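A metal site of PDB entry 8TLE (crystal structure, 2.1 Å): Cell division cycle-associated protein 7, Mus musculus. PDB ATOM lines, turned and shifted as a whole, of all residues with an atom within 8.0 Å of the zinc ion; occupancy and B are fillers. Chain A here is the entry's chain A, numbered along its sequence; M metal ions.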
ATOM      1  N   HIS A  44      19.072  32.123  10.099  1.00  0.00           N
ATOM      2  CA  HIS A  44      18.698  32.247  11.499  1.00  0.00           C
ATOM      3  C   HIS A  44      19.851  31.861  12.424  1.00  0.00           C
ATOM      4  O   HIS A  44      19.993  32.427  13.508  1.00  0.00           O
ATOM      5  CB  HIS A  44      17.469  31.393  11.804  1.00  0.00           C
ATOM      6  CG  HIS A  44      17.171  31.261  13.264  1.00  0.00           C
ATOM      7  ND1 HIS A  44      16.788  32.320  14.049  1.00  0.00           N
ATOM      8  CD2 HIS A  44      17.202  30.179  14.088  1.00  0.00           C
ATOM      9  CE1 HIS A  44      16.593  31.903  15.292  1.00  0.00           C
ATOM     10  NE2 HIS A  44      16.838  30.610  15.330  1.00  0.00           N
ATOM     11  N   GLN A  45      20.676  30.898  12.009  1.00  0.00           N
ATOM     12  CA  GLN A  45      21.732  30.381  12.863  1.00  0.00           C
ATOM     13  C   GLN A  45      22.907  31.355  12.962  1.00  0.00           C
ATOM     14  O   GLN A  45      23.252  31.816  14.050  1.00  0.00           O
ATOM     15  CB  GLN A  45      22.202  29.017  12.362  1.00  0.00           C
ATOM     16  CG  GLN A  45      23.156  28.300  13.290  1.00  0.00           C
ATOM     17  CD  GLN A  45      22.446  27.586  14.424  1.00  0.00           C
ATOM     18  OE1 GLN A  45      21.236  27.349  14.372  1.00  0.00           O
ATOM     19  NE2 GLN A  45      23.191  27.240  15.466  1.00  0.00           N
ATOM     20  N   ARG A  47      23.143  34.344  11.443  1.00  0.00           N
ATOM     21  CA  ARG A  47      22.702  35.745  11.389  1.00  0.00           C
ATOM     22  C   ARG A  47      23.518  36.561  10.383  1.00  0.00           C
ATOM     23  O   ARG A  47      23.936  37.681  10.662  1.00  0.00           O
ATOM     24  CB  ARG A  47      22.753  36.379  12.781  1.00  0.00           C
ATOM     25  CG  ARG A  47      21.899  35.635  13.807  1.00  0.00           C
ATOM     26  CD  ARG A  47      21.823  36.364  15.135  1.00  0.00           C
ATOM     27  NE  ARG A  47      23.045  36.249  15.918  1.00  0.00           N
ATOM     28  CZ  ARG A  47      23.278  35.271  16.790  1.00  0.00           C
ATOM     29  NH1 ARG A  47      22.397  34.307  16.997  1.00  0.00           N
ATOM     30  NH2 ARG A  47      24.421  35.278  17.475  1.00  0.00           N
ATOM     31  N   ARG A  66      12.965  32.880  10.896  1.00  0.00           N
ATOM     32  CA  ARG A  66      13.582  31.899  11.793  1.00  0.00           C
ATOM     33  C   ARG A  66      13.700  30.527  11.151  1.00  0.00           C
ATOM     34  O   ARG A  66      14.412  29.670  11.693  1.00  0.00           O
ATOM     35  CB  ARG A  66      12.803  31.808  13.103  1.00  0.00           C
ATOM     36  CG  ARG A  66      11.446  31.130  12.994  1.00  0.00           C
ATOM     37  CD  ARG A  66      10.812  31.008  14.374  1.00  0.00           C
ATOM     38  NE  ARG A  66       9.757  30.001  14.406  1.00  0.00           N
ATOM     39  CZ  ARG A  66       9.198  29.544  15.520  1.00  0.00           C
ATOM     40  NH1 ARG A  66       9.576  29.980  16.710  1.00  0.00           N
ATOM     41  NH2 ARG A  66       8.249  28.616  15.437  1.00  0.00           N
ATOM     42  N   PHE A  69      17.902  28.797   7.004  1.00  0.00           N
ATOM     43  CA  PHE A  69      19.210  28.323   7.407  1.00  0.00           C
ATOM     44  C   PHE A  69      20.094  28.154   6.180  1.00  0.00           C
ATOM     45  O   PHE A  69      19.648  27.636   5.156  1.00  0.00           O
ATOM     46  CB  PHE A  69      19.121  26.996   8.172  1.00  0.00           C
ATOM     47  CG  PHE A  69      18.519  27.129   9.542  1.00  0.00           C
ATOM     48  CD1 PHE A  69      17.153  27.262   9.713  1.00  0.00           C
ATOM     49  CD2 PHE A  69      19.330  27.134  10.668  1.00  0.00           C
ATOM     50  CE1 PHE A  69      16.604  27.389  10.971  1.00  0.00           C
ATOM     51  CE2 PHE A  69      18.796  27.254  11.933  1.00  0.00           C
ATOM     52  CZ  PHE A  69      17.430  27.384  12.087  1.00  0.00           C
ATOM     53  N   TYR A  78      23.106  20.720  12.562  1.00  0.00           N
ATOM     54  CA  TYR A  78      21.999  19.784  12.614  1.00  0.00           C
ATOM     55  C   TYR A  78      22.204  18.535  11.775  1.00  0.00           C
ATOM     56  O   TYR A  78      21.327  17.656  11.782  1.00  0.00           O
ATOM     57  CB  TYR A  78      20.695  20.477  12.178  1.00  0.00           C
ATOM     58  CG  TYR A  78      20.390  21.717  12.986  1.00  0.00           C
ATOM     59  CD1 TYR A  78      20.746  22.984  12.514  1.00  0.00           C
ATOM     60  CD2 TYR A  78      19.785  21.628  14.226  1.00  0.00           C
ATOM     61  CE1 TYR A  78      20.472  24.109  13.257  1.00  0.00           C
ATOM     62  CE2 TYR A  78      19.511  22.745  14.976  1.00  0.00           C
ATOM     63  CZ  TYR A  78      19.861  23.997  14.489  1.00  0.00           C
ATOM     64  OH  TYR A  78      19.593  25.117  15.226  1.00  0.00           O
ATOM     65  N   PRO A  94      14.455  23.994  12.794  1.00  0.00           N
ATOM     66  CA  PRO A  94      14.774  23.614  14.180  1.00  0.00           C
ATOM     67  C   PRO A  94      14.039  24.462  15.206  1.00  0.00           C
ATOM     68  O   PRO A  94      13.637  23.928  16.257  1.00  0.00           O
ATOM     69  CB  PRO A  94      16.291  23.822  14.251  1.00  0.00           C
ATOM     70  CG  PRO A  94      16.754  23.588  12.859  1.00  0.00           C
ATOM     71  CD  PRO A  94      15.660  24.118  11.963  1.00  0.00           C
ATOM     72  N   PRO A  95      13.836  25.775  14.983  1.00  0.00           N
ATOM     73  CA  PRO A  95      12.975  26.512  15.918  1.00  0.00           C
ATOM     74  C   PRO A  95      11.572  25.944  16.027  1.00  0.00           C
ATOM     75  O   PRO A  95      10.995  25.930  17.127  1.00  0.00           O
ATOM     76  CB  PRO A  95      12.975  27.932  15.328  1.00  0.00           C
ATOM     77  CG  PRO A  95      14.279  28.043  14.678  1.00  0.00           C
ATOM     78  CD  PRO A  95      14.539  26.698  14.069  1.00  0.00           C
ATOM     79  N   ILE A  99      14.451  22.327  18.603  1.00  0.00           N
ATOM     80  CA  ILE A  99      15.780  21.756  18.686  1.00  0.00           C
ATOM     81  C   ILE A  99      16.857  22.738  18.237  1.00  0.00           C
ATOM     82  O   ILE A  99      18.006  22.341  18.025  1.00  0.00           O
ATOM     83  CB  ILE A  99      15.876  20.442  17.890  1.00  0.00           C
ATOM     84  CG1 ILE A  99      15.671  20.711  16.394  1.00  0.00           C
ATOM     85  CG2 ILE A  99      14.851  19.433  18.394  1.00  0.00           C
ATOM     86  CD1 ILE A  99      15.741  19.473  15.535  1.00  0.00           C
ATOM     87  N   CYS A 100      16.509  24.016  18.076  1.00  0.00           N
ATOM     88  CA  CYS A 100      17.479  25.003  17.612  1.00  0.00           C
ATOM     89  C   CYS A 100      18.541  25.246  18.678  1.00  0.00           C
ATOM     90  O   CYS A 100      18.226  25.469  19.845  1.00  0.00           O
ATOM     91  CB  CYS A 100      16.769  26.308  17.247  1.00  0.00           C
ATOM     92  SG  CYS A 100      17.853  27.538  16.463  1.00  0.00           S
ATOM     93  N   ASN A 101      19.803  25.192  18.264  1.00  0.00           N
ATOM     94  CA  ASN A 101      20.931  25.387  19.160  1.00  0.00           C
ATOM     95  C   ASN A 101      21.683  26.682  18.889  1.00  0.00           C
ATOM     96  O   ASN A 101      22.873  26.790  19.212  1.00  0.00           O
ATOM     97  CB  ASN A 101      21.897  24.195  19.074  1.00  0.00           C
ATOM     98  CG  ASN A 101      22.299  23.876  17.656  1.00  0.00           C
ATOM     99  OD1 ASN A 101      23.062  24.622  17.030  1.00  0.00           O
ATOM    100  ND2 ASN A 101      21.809  22.761  17.127  1.00  0.00           N
ATOM    101  N   CYS A 102      21.020  27.674  18.296  1.00  0.00           N
ATOM    102  CA  CYS A 102      21.655  28.963  18.099  1.00  0.00           C
ATOM    103  C   CYS A 102      21.871  29.661  19.430  1.00  0.00           C
ATOM    104  O   CYS A 102      21.278  29.296  20.455  1.00  0.00           O
ATOM    105  CB  CYS A 102      20.821  29.841  17.155  1.00  0.00           C
ATOM    106  SG  CYS A 102      19.392  30.638  17.922  1.00  0.00           S
ATOM    107  N   SER A 103      22.743  30.670  19.415  1.00  0.00           N
ATOM    108  CA  SER A 103      23.157  31.315  20.660  1.00  0.00           C
ATOM    109  C   SER A 103      21.978  31.902  21.435  1.00  0.00           C
ATOM    110  O   SER A 103      22.012  31.961  22.664  1.00  0.00           O
ATOM    111  CB  SER A 103      24.186  32.413  20.365  1.00  0.00           C
ATOM    112  OG  SER A 103      23.627  33.427  19.555  1.00  0.00           O
ATOM    113  N   PHE A 104      20.930  32.334  20.722  1.00  0.00           N
ATOM    114  CA  PHE A 104      19.755  32.893  21.395  1.00  0.00           C
ATOM    115  C   PHE A 104      18.796  31.795  21.859  1.00  0.00           C
ATOM    116  O   PHE A 104      18.281  31.857  22.974  1.00  0.00           O
ATOM    117  CB  PHE A 104      19.046  33.881  20.483  1.00  0.00           C
ATOM    118  CG  PHE A 104      17.755  34.401  21.037  1.00  0.00           C
ATOM    119  CD1 PHE A 104      17.756  35.395  22.013  1.00  0.00           C
ATOM    120  CD2 PHE A 104      16.542  33.915  20.597  1.00  0.00           C
ATOM    121  CE1 PHE A 104      16.572  35.878  22.535  1.00  0.00           C
ATOM    122  CE2 PHE A 104      15.343  34.404  21.112  1.00  0.00           C
ATOM    123  CZ  PHE A 104      15.373  35.383  22.084  1.00  0.00           C
ATOM    124  N   CYS A 105      18.552  30.804  21.005  1.00  0.00           N
ATOM    125  CA  CYS A 105      17.578  29.769  21.319  1.00  0.00           C
ATOM    126  C   CYS A 105      18.066  28.764  22.346  1.00  0.00           C
ATOM    127  O   CYS A 105      17.244  28.130  23.021  1.00  0.00           O
ATOM    128  CB  CYS A 105      17.153  29.036  20.041  1.00  0.00           C
ATOM    129  SG  CYS A 105      16.193  30.033  18.883  1.00  0.00           S
ATOM    130  N   ARG A 106      19.388  28.577  22.482  1.00  0.00           N
ATOM    131  CA  ARG A 106      19.894  27.550  23.383  1.00  0.00           C
ATOM    132  C   ARG A 106      19.689  27.926  24.845  1.00  0.00           C
ATOM    133  O   ARG A 106      19.392  27.067  25.680  1.00  0.00           O
ATOM    134  CB  ARG A 106      21.361  27.262  23.087  1.00  0.00           C
ATOM    135  CG  ARG A 106      22.350  28.353  23.494  1.00  0.00           C
ATOM    136  CD  ARG A 106      23.779  27.888  23.319  1.00  0.00           C
ATOM    137  NE  ARG A 106      24.101  27.646  21.915  1.00  0.00           N
ATOM    138  CZ  ARG A 106      24.983  28.351  21.222  1.00  0.00           C
ATOM    139  NH1 ARG A 106      25.656  29.349  21.775  1.00  0.00           N
ATOM    140  NH2 ARG A 106      25.213  28.033  19.949  1.00  0.00           N
HETATM  141 ZN    ZN M   1      17.494  29.730  17.051  1.00  0.00          ZN
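The zinc ion is bound by NE2 of His 44 (2.0 Å), SG of Cys 105 (2.3 Å), SG of Cys 102 (2.3 Å) and SG of Cys 100 (2.3 Å). The zinc ion has four donor atoms within binding distance.
The side-chain sulfur (SG) of Cys 102 sits close to the backbone NH (N) of Phe 104 (3.6 Å). The side-chain sulfur (SG) of Cys 100 lies close to the side-chain hydroxyl (OH) of Tyr 78, 3.2 Å away. The backbone NH (N) of Cys 100 is in hydrogen-bond range of the backbone carbonyl oxygen (O) of Pro 94, 3.4 Å away.
Within 4 Å of the zinc ion: His 44, Cys 100, Cys 102 and Cys 105. The nearest printed residue that does not touch the zinc ion is Pro 95 (4.3 Å).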
